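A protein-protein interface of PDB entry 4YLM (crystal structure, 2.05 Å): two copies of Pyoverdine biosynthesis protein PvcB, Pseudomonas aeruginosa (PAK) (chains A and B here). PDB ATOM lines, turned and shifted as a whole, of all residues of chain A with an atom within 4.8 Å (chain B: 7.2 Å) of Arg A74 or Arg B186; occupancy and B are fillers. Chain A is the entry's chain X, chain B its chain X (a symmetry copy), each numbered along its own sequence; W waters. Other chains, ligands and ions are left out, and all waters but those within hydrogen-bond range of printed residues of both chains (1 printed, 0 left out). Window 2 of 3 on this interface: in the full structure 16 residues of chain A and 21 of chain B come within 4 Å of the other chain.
Tyr A75 touches Glu B191 (N to CG, 3.9 Å).
Asp A78 touches Arg B189 (CB to O, 3.3 Å).
Asp A78 touches Arg B190 (OD2 to CG, 3.6 Å).
Printed residues of chain A that touch a printed residue of chain B: Ser A71, Arg A74, Tyr A75 and Asp A78.
Among the printed residues, Asp or Glu carboxylates within 4 Å of a Lys or Arg side-chain nitrogen of the other chain: Arg A74 with Glu B191 (2.7 Å).
The side-chain hydroxyl of Ser A71 lies within hydrogen-bond range of the side-chain carboxylate of Glu B191 (2.6 Å).
NE of Arg A74 lies within salt-bridge range of OE2 of Glu B191 (2.7 Å).
NH2 of Arg A74 sits close to NH1 of Arg B186, 3.3 Å away.
The guanidinium group of Arg B186 lies within salt-bridge range of the side-chain carboxylate of Glu B191 (3.6 Å).
The backbone NH (N) of Arg B189 sits at hydrogen-bond distance from a ring nitrogen (ND1) of His B187.
A ring nitrogen (ND1) of His B187 is in hydrogen-bond range of the backbone NH of Arg B190 (2.9 Å).
Water W1 bridges O of Arg B189 (2.6 Å) and O of Arg A74 (2.7 Å).
Arg A74 touches two residues of chain B.
Of the printed residues of chain A, Arg B186 touches Arg A74.
Of the printed residues of chain A, Arg B189 touches Asp A78 (3.3 Å).
Of the printed residues of chain A, Glu B191 touches Ser A71, Arg A74 and Tyr A75.
Of the printed residues of chain B, Asp A78 touches Arg B189 (3.3 Å) and Arg B190 (3.6 Å).
Val B184 touches none of the printed residues of chain A.
Leu B257 touches none of the printed residues of chain A.
The nearest residue of chain B that does not touch Arg A74 is Arg B189 (4.3 Å).
The nearest printed residue of chain A that does not touch Arg B186 is Ser A71 (5.9 Å).
The nearest printed residue of chain A that does not touch Arg B189 is Arg A74 (4.3 Å).
No position is printed for both chains.
Of the 6 pairs that touch across the chains among the printed residues, none has its exchanged pair printed and touching as well.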
ATOM      1  N   GLU A  70      19.766  -3.292   1.805  1.00  0.00           N
ATOM      2  CA  GLU A  70      20.663  -2.160   1.927  1.00  0.00           C
ATOM      3  C   GLU A  70      22.067  -2.635   2.333  1.00  0.00           C
ATOM      4  O   GLU A  70      23.068  -2.169   1.790  1.00  0.00           O
ATOM      5  CB  GLU A  70      20.114  -1.172   2.965  1.00  0.00           C
ATOM      6  CG  GLU A  70      18.862  -0.391   2.529  1.00  0.00           C
ATOM      7  CD  GLU A  70      17.530  -1.160   2.668  1.00  0.00           C
ATOM      8  OE1 GLU A  70      17.524  -2.345   3.070  1.00  0.00           O
ATOM      9  OE2 GLU A  70      16.472  -0.560   2.363  1.00  0.00           O
ATOM     10  N   SER A  71      22.127  -3.551   3.297  1.00  0.00           N
ATOM     11  CA  SER A  71      23.393  -4.115   3.748  1.00  0.00           C
ATOM     12  C   SER A  71      24.068  -4.876   2.605  1.00  0.00           C
ATOM     13  O   SER A  71      25.257  -4.691   2.337  1.00  0.00           O
ATOM     14  CB  SER A  71      23.163  -5.040   4.945  1.00  0.00           C
ATOM     15  OG  SER A  71      24.391  -5.570   5.418  1.00  0.00           O
ATOM     16  N   LEU A  72      23.303  -5.714   1.910  1.00  0.00           N
ATOM     17  CA  LEU A  72      23.837  -6.413   0.740  1.00  0.00           C
ATOM     18  C   LEU A  72      24.395  -5.424  -0.268  1.00  0.00           C
ATOM     19  O   LEU A  72      25.463  -5.625  -0.812  1.00  0.00           O
ATOM     20  CB  LEU A  72      22.767  -7.296   0.082  1.00  0.00           C
ATOM     21  CG  LEU A  72      23.111  -8.012  -1.230  1.00  0.00           C
ATOM     22  CD1 LEU A  72      24.317  -8.939  -1.083  1.00  0.00           C
ATOM     23  CD2 LEU A  72      21.892  -8.793  -1.732  1.00  0.00           C
ATOM     24  N   THR A  73      23.669  -4.343  -0.514  1.00  0.00           N
ATOM     25  CA  THR A  73      24.099  -3.357  -1.496  1.00  0.00           C
ATOM     26  C   THR A  73      25.441  -2.714  -1.115  1.00  0.00           C
ATOM     27  O   THR A  73      26.338  -2.610  -1.948  1.00  0.00           O
ATOM     28  CB  THR A  73      23.011  -2.268  -1.675  1.00  0.00           C
ATOM     29  OG1 THR A  73      21.820  -2.872  -2.190  1.00  0.00           O
ATOM     30  CG2 THR A  73      23.464  -1.198  -2.641  1.00  0.00           C
ATOM     31  N   ARG A  74      25.573  -2.274   0.131  1.00  0.00           N
ATOM     32  CA  ARG A  74      26.829  -1.671   0.576  1.00  0.00           C
ATOM     33  C   ARG A  74      27.984  -2.670   0.441  1.00  0.00           C
ATOM     34  O   ARG A  74      29.082  -2.315  -0.009  1.00  0.00           O
ATOM     35  CB  ARG A  74      26.721  -1.160   2.021  1.00  0.00           C
ATOM     36  CG  ARG A  74      25.774   0.040   2.196  1.00  0.00           C
ATOM     37  CD  ARG A  74      25.849   0.623   3.607  1.00  0.00           C
ATOM     38  NE  ARG A  74      25.436  -0.330   4.630  1.00  0.00           N
ATOM     39  CZ  ARG A  74      24.189  -0.458   5.076  1.00  0.00           C
ATOM     40  NH1 ARG A  74      23.228   0.318   4.591  1.00  0.00           N
ATOM     41  NH2 ARG A  74      23.907  -1.357   6.010  1.00  0.00           N
ATOM     42  N   TYR A  75      27.733  -3.922   0.819  1.00  0.00           N
ATOM     43  CA  TYR A  75      28.746  -4.955   0.655  1.00  0.00           C
ATOM     44  C   TYR A  75      29.175  -5.069  -0.795  1.00  0.00           C
ATOM     45  O   TYR A  75      30.370  -5.159  -1.089  1.00  0.00           O
ATOM     46  CB  TYR A  75      28.256  -6.318   1.142  1.00  0.00           C
ATOM     47  CG  TYR A  75      29.203  -7.435   0.758  1.00  0.00           C
ATOM     48  CD1 TYR A  75      30.301  -7.743   1.554  1.00  0.00           C
ATOM     49  CD2 TYR A  75      29.010  -8.167  -0.410  1.00  0.00           C
ATOM     50  CE1 TYR A  75      31.173  -8.756   1.202  1.00  0.00           C
ATOM     51  CE2 TYR A  75      29.878  -9.178  -0.768  1.00  0.00           C
ATOM     52  CZ  TYR A  75      30.962  -9.466   0.041  1.00  0.00           C
ATOM     53  OH  TYR A  75      31.840 -10.472  -0.312  1.00  0.00           O
ATOM     54  N   CYS A  76      28.204  -5.080  -1.707  1.00  0.00           N
ATOM     55  CA  CYS A  76      28.526  -5.261  -3.121  1.00  0.00           C
ATOM     56  C   CYS A  76      29.283  -4.081  -3.707  1.00  0.00           C
ATOM     57  O   CYS A  76      30.105  -4.269  -4.608  1.00  0.00           O
ATOM     58  CB  CYS A  76      27.279  -5.565  -3.958  1.00  0.00           C
ATOM     59  SG  CYS A  76      26.620  -7.224  -3.670  1.00  0.00           S
ATOM     60  N   HIS A  77      29.016  -2.874  -3.198  1.00  0.00           N
ATOM     61  CA  HIS A  77      29.764  -1.692  -3.635  1.00  0.00           C
ATOM     62  C   HIS A  77      31.236  -1.796  -3.210  1.00  0.00           C
ATOM     63  O   HIS A  77      32.120  -1.253  -3.879  1.00  0.00           O
ATOM     64  CB  HIS A  77      29.146  -0.394  -3.088  1.00  0.00           C
ATOM     65  CG  HIS A  77      27.899   0.038  -3.798  1.00  0.00           C
ATOM     66  ND1 HIS A  77      27.866   0.305  -5.150  1.00  0.00           N
ATOM     67  CD2 HIS A  77      26.644   0.270  -3.339  1.00  0.00           C
ATOM     68  CE1 HIS A  77      26.644   0.673  -5.495  1.00  0.00           C
ATOM     69  NE2 HIS A  77      25.883   0.657  -4.415  1.00  0.00           N
ATOM     70  N   ASP A  78      31.501  -2.467  -2.085  1.00  0.00           N
ATOM     71  CA  ASP A  78      32.888  -2.716  -1.680  1.00  0.00           C
ATOM     72  C   ASP A  78      33.485  -3.841  -2.519  1.00  0.00           C
ATOM     73  O   ASP A  78      34.660  -3.825  -2.862  1.00  0.00           O
ATOM     74  CB  ASP A  78      32.983  -3.100  -0.198  1.00  0.00           C
ATOM     75  CG  ASP A  78      34.429  -3.149   0.298  1.00  0.00           C
ATOM     76  OD1 ASP A  78      35.124  -2.120   0.175  1.00  0.00           O
ATOM     77  OD2 ASP A  78      34.882  -4.210   0.790  1.00  0.00           O
ATOM     78  N   PRO B 182      27.843   4.179  18.136  1.00  0.00           N
ATOM     79  CA  PRO B 182      27.124   3.083  18.790  1.00  0.00           C
ATOM     80  C   PRO B 182      28.142   2.048  19.253  1.00  0.00           C
ATOM     81  O   PRO B 182      29.179   1.879  18.596  1.00  0.00           O
ATOM     82  CB  PRO B 182      26.275   2.492  17.659  1.00  0.00           C
ATOM     83  CG  PRO B 182      26.225   3.554  16.597  1.00  0.00           C
ATOM     84  CD  PRO B 182      27.494   4.322  16.715  1.00  0.00           C
ATOM     85  N   VAL B 184      27.581  -1.215  19.293  1.00  0.00           N
ATOM     86  CA  VAL B 184      27.497  -2.240  18.258  1.00  0.00           C
ATOM     87  C   VAL B 184      27.418  -1.558  16.897  1.00  0.00           C
ATOM     88  O   VAL B 184      26.488  -0.800  16.628  1.00  0.00           O
ATOM     89  CB  VAL B 184      26.278  -3.177  18.486  1.00  0.00           C
ATOM     90  CG1 VAL B 184      26.192  -4.246  17.397  1.00  0.00           C
ATOM     91  CG2 VAL B 184      26.360  -3.822  19.874  1.00  0.00           C
ATOM     92  N   GLU B 185      28.409  -1.809  16.044  1.00  0.00           N
ATOM     93  CA  GLU B 185      28.472  -1.156  14.741  1.00  0.00           C
ATOM     94  C   GLU B 185      28.459  -2.194  13.627  1.00  0.00           C
ATOM     95  O   GLU B 185      28.472  -3.395  13.892  1.00  0.00           O
ATOM     96  CB  GLU B 185      29.750  -0.313  14.626  1.00  0.00           C
ATOM     97  CG  GLU B 185      29.569   1.175  14.886  1.00  0.00           C
ATOM     98  CD  GLU B 185      28.844   1.875  13.752  1.00  0.00           C
ATOM     99  OE1 GLU B 185      28.921   3.117  13.690  1.00  0.00           O
ATOM    100  OE2 GLU B 185      28.194   1.188  12.929  1.00  0.00           O
ATOM    101  N   ARG B 186      28.425  -1.726  12.385  1.00  0.00           N
ATOM    102  CA  ARG B 186      28.708  -2.582  11.246  1.00  0.00           C
ATOM    103  C   ARG B 186      30.085  -2.199  10.715  1.00  0.00           C
ATOM    104  O   ARG B 186      30.485  -1.028  10.778  1.00  0.00           O
ATOM    105  CB  ARG B 186      27.645  -2.414  10.157  1.00  0.00           C
ATOM    106  CG  ARG B 186      27.602  -1.034   9.538  1.00  0.00           C
ATOM    107  CD  ARG B 186      26.462  -0.951   8.544  1.00  0.00           C
ATOM    108  NE  ARG B 186      26.428   0.313   7.813  1.00  0.00           N
ATOM    109  CZ  ARG B 186      25.384   1.140   7.800  1.00  0.00           C
ATOM    110  NH1 ARG B 186      24.287   0.845   8.491  1.00  0.00           N
ATOM    111  NH2 ARG B 186      25.434   2.266   7.095  1.00  0.00           N
ATOM    112  N   HIS B 187      30.832  -3.178  10.226  1.00  0.00           N
ATOM    113  CA  HIS B 187      32.110  -2.854   9.614  1.00  0.00           C
ATOM    114  C   HIS B 187      31.830  -1.854   8.503  1.00  0.00           C
ATOM    115  O   HIS B 187      30.918  -2.057   7.691  1.00  0.00           O
ATOM    116  CB  HIS B 187      32.783  -4.105   9.058  1.00  0.00           C
ATOM    117  CG  HIS B 187      34.161  -3.857   8.533  1.00  0.00           C
ATOM    118  ND1 HIS B 187      34.391  -3.234   7.324  1.00  0.00           N
ATOM    119  CD2 HIS B 187      35.378  -4.127   9.057  1.00  0.00           C
ATOM    120  CE1 HIS B 187      35.692  -3.151   7.117  1.00  0.00           C
ATOM    121  NE2 HIS B 187      36.317  -3.691   8.149  1.00  0.00           N
ATOM    122  N   PRO B 188      32.593  -0.755   8.471  1.00  0.00           N
ATOM    123  CA  PRO B 188      32.266   0.360   7.572  1.00  0.00           C
ATOM    124  C   PRO B 188      32.501   0.084   6.083  1.00  0.00           C
ATOM    125  O   PRO B 188      32.091   0.900   5.260  1.00  0.00           O
ATOM    126  CB  PRO B 188      33.175   1.498   8.075  1.00  0.00           C
ATOM    127  CG  PRO B 188      34.342   0.779   8.725  1.00  0.00           C
ATOM    128  CD  PRO B 188      33.718  -0.443   9.370  1.00  0.00           C
ATOM    129  N   ARG B 189      33.132  -1.032   5.733  1.00  0.00           N
ATOM    130  CA  ARG B 189      33.263  -1.394   4.321  1.00  0.00           C
ATOM    131  C   ARG B 189      32.625  -2.746   4.032  1.00  0.00           C
ATOM    132  O   ARG B 189      32.068  -2.952   2.962  1.00  0.00           O
ATOM    133  CB  ARG B 189      34.740  -1.409   3.888  1.00  0.00           C
ATOM    134  CG  ARG B 189      35.346  -0.013   3.777  1.00  0.00           C
ATOM    135  CD  ARG B 189      34.644   0.749   2.648  1.00  0.00           C
ATOM    136  NE  ARG B 189      34.731   2.200   2.811  1.00  0.00           N
ATOM    137  CZ  ARG B 189      35.776   2.917   2.418  1.00  0.00           C
ATOM    138  NH1 ARG B 189      36.798   2.306   1.842  1.00  0.00           N
ATOM    139  NH2 ARG B 189      35.791   4.239   2.591  1.00  0.00           N
ATOM    140  N   ARG B 190      32.680  -3.648   5.007  1.00  0.00           N
ATOM    141  CA  ARG B 190      32.385  -5.052   4.749  1.00  0.00           C
ATOM    142  C   ARG B 190      31.169  -5.568   5.509  1.00  0.00           C
ATOM    143  O   ARG B 190      30.853  -6.757   5.452  1.00  0.00           O
ATOM    144  CB  ARG B 190      33.625  -5.901   5.041  1.00  0.00           C
ATOM    145  CG  ARG B 190      34.788  -5.617   4.082  1.00  0.00           C
ATOM    146  CD  ARG B 190      35.930  -6.589   4.342  1.00  0.00           C
ATOM    147  NE  ARG B 190      36.699  -6.258   5.541  1.00  0.00           N
ATOM    148  CZ  ARG B 190      37.232  -7.161   6.355  1.00  0.00           C
ATOM    149  NH1 ARG B 190      37.030  -8.454   6.130  1.00  0.00           N
ATOM    150  NH2 ARG B 190      37.968  -6.781   7.399  1.00  0.00           N
ATOM    151  N   GLU B 191      30.508  -4.663   6.231  1.00  0.00           N
ATOM    152  CA  GLU B 191      29.163  -4.893   6.776  1.00  0.00           C
ATOM    153  C   GLU B 191      29.012  -5.759   8.022  1.00  0.00           C
ATOM    154  O   GLU B 191      28.009  -5.631   8.727  1.00  0.00           O
ATOM    155  CB  GLU B 191      28.198  -5.395   5.690  1.00  0.00           C
ATOM    156  CG  GLU B 191      27.796  -4.325   4.705  1.00  0.00           C
ATOM    157  CD  GLU B 191      26.959  -3.238   5.367  1.00  0.00           C
ATOM    158  OE1 GLU B 191      25.909  -3.567   5.968  1.00  0.00           O
ATOM    159  OE2 GLU B 191      27.370  -2.061   5.303  1.00  0.00           O
ATOM    160  N   PHE B 192      29.969  -6.634   8.313  1.00  0.00           N
ATOM    161  CA  PHE B 192      29.754  -7.571   9.422  1.00  0.00           C
ATOM    162  C   PHE B 192      29.741  -6.861  10.772  1.00  0.00           C
ATOM    163  O   PHE B 192      30.322  -5.788  10.911  1.00  0.00           O
ATOM    164  CB  PHE B 192      30.773  -8.715   9.402  1.00  0.00           C
ATOM    165  CG  PHE B 192      32.212  -8.263   9.485  1.00  0.00           C
ATOM    166  CD1 PHE B 192      32.834  -8.111  10.711  1.00  0.00           C
ATOM    167  CD2 PHE B 192      32.943  -8.014   8.327  1.00  0.00           C
ATOM    168  CE1 PHE B 192      34.176  -7.707  10.792  1.00  0.00           C
ATOM    169  CE2 PHE B 192      34.269  -7.609   8.389  1.00  0.00           C
ATOM    170  CZ  PHE B 192      34.891  -7.461   9.625  1.00  0.00           C
ATOM    171  N   PRO B 193      29.059  -7.450  11.770  1.00  0.00           N
ATOM    172  CA  PRO B 193      28.972  -6.820  13.095  1.00  0.00           C
ATOM    173  C   PRO B 193      30.313  -6.681  13.804  1.00  0.00           C
ATOM    174  O   PRO B 193      31.107  -7.627  13.867  1.00  0.00           O
ATOM    175  CB  PRO B 193      28.050  -7.774  13.881  1.00  0.00           C
ATOM    176  CG  PRO B 193      27.206  -8.422  12.829  1.00  0.00           C
ATOM    177  CD  PRO B 193      28.147  -8.606  11.649  1.00  0.00           C
ATOM    178  N   ILE B 194      30.565  -5.485  14.322  1.00  0.00           N
ATOM    179  CA  ILE B 194      31.761  -5.220  15.112  1.00  0.00           C
ATOM    180  C   ILE B 194      31.356  -4.413  16.349  1.00  0.00           C
ATOM    181  O   ILE B 194      30.203  -4.006  16.478  1.00  0.00           O
ATOM    182  CB  ILE B 194      32.777  -4.374  14.322  1.00  0.00           C
ATOM    183  CG1 ILE B 194      32.115  -3.070  13.850  1.00  0.00           C
ATOM    184  CG2 ILE B 194      33.382  -5.183  13.123  1.00  0.00           C
ATOM    185  CD1 ILE B 194      33.128  -2.008  13.328  1.00  0.00           C
ATOM    186  N   LEU B 195      32.309  -4.177  17.242  1.00  0.00           N
ATOM    187  CA  LEU B 195      32.112  -3.231  18.331  1.00  0.00           C
ATOM    188  C   LEU B 195      33.014  -2.021  18.110  1.00  0.00           C
ATOM    189  O   LEU B 195      34.151  -2.156  17.638  1.00  0.00           O
ATOM    190  CB  LEU B 195      32.443  -3.878  19.676  1.00  0.00           C
ATOM    191  CG  LEU B 195      31.689  -5.154  20.070  1.00  0.00           C
ATOM    192  CD1 LEU B 195      32.242  -5.710  21.366  1.00  0.00           C
ATOM    193  CD2 LEU B 195      30.186  -4.878  20.205  1.00  0.00           C
ATOM    194  N   ARG B 196      32.502  -0.839  18.439  1.00  0.00           N
ATOM    195  CA  ARG B 196      33.350   0.352  18.566  1.00  0.00           C
ATOM    196  C   ARG B 196      33.167   0.846  20.000  1.00  0.00           C
ATOM    197  O   ARG B 196      32.090   1.281  20.373  1.00  0.00           O
ATOM    198  CB  ARG B 196      32.944   1.440  17.565  1.00  0.00           C
ATOM    199  CG  ARG B 196      33.171   1.073  16.100  1.00  0.00           C
ATOM    200  CD  ARG B 196      34.665   0.982  15.730  1.00  0.00           C
ATOM    201  NE  ARG B 196      35.264  -0.303  16.098  1.00  0.00           N
ATOM    202  CZ  ARG B 196      36.508  -0.670  15.782  1.00  0.00           C
ATOM    203  NH1 ARG B 196      37.297   0.150  15.096  1.00  0.00           N
ATOM    204  NH2 ARG B 196      36.969  -1.860  16.151  1.00  0.00           N
ATOM    205  N   LEU B 257      39.855  -1.651  11.827  1.00  0.00           N
ATOM    206  CA  LEU B 257      38.405  -1.493  11.650  1.00  0.00           C
ATOM    207  C   LEU B 257      37.608  -2.563  12.395  1.00  0.00           C
ATOM    208  O   LEU B 257      36.401  -2.417  12.600  1.00  0.00           O
ATOM    209  CB  LEU B 257      38.017  -1.486  10.155  1.00  0.00           C
ATOM    210  CG  LEU B 257      38.745  -0.451   9.278  1.00  0.00           C
ATOM    211  CD1 LEU B 257      38.199  -0.466   7.844  1.00  0.00           C
ATOM    212  CD2 LEU B 257      38.623   0.964   9.885  1.00  0.00           C
ATOM    213  N   HIS B 289      32.138   8.873  12.944  1.00  0.00           N
ATOM    214  CA  HIS B 289      31.795   9.137  14.336  1.00  0.00           C
ATOM    215  C   HIS B 289      32.260  10.500  14.844  1.00  0.00           C
ATOM    216  O   HIS B 289      31.917  10.903  15.958  1.00  0.00           O
ATOM    217  CB  HIS B 289      32.349   8.024  15.224  1.00  0.00           C
ATOM    218  CG  HIS B 289      31.897   6.656  14.815  1.00  0.00           C
ATOM    219  ND1 HIS B 289      32.773   5.610  14.618  1.00  0.00           N
ATOM    220  CD2 HIS B 289      30.660   6.168  14.563  1.00  0.00           C
ATOM    221  CE1 HIS B 289      32.090   4.532  14.269  1.00  0.00           C
ATOM    222  NE2 HIS B 289      30.807   4.844  14.226  1.00  0.00           N
HETATM  223  O   HOH W   1      30.691  -1.119   1.750  1.00  0.00           O
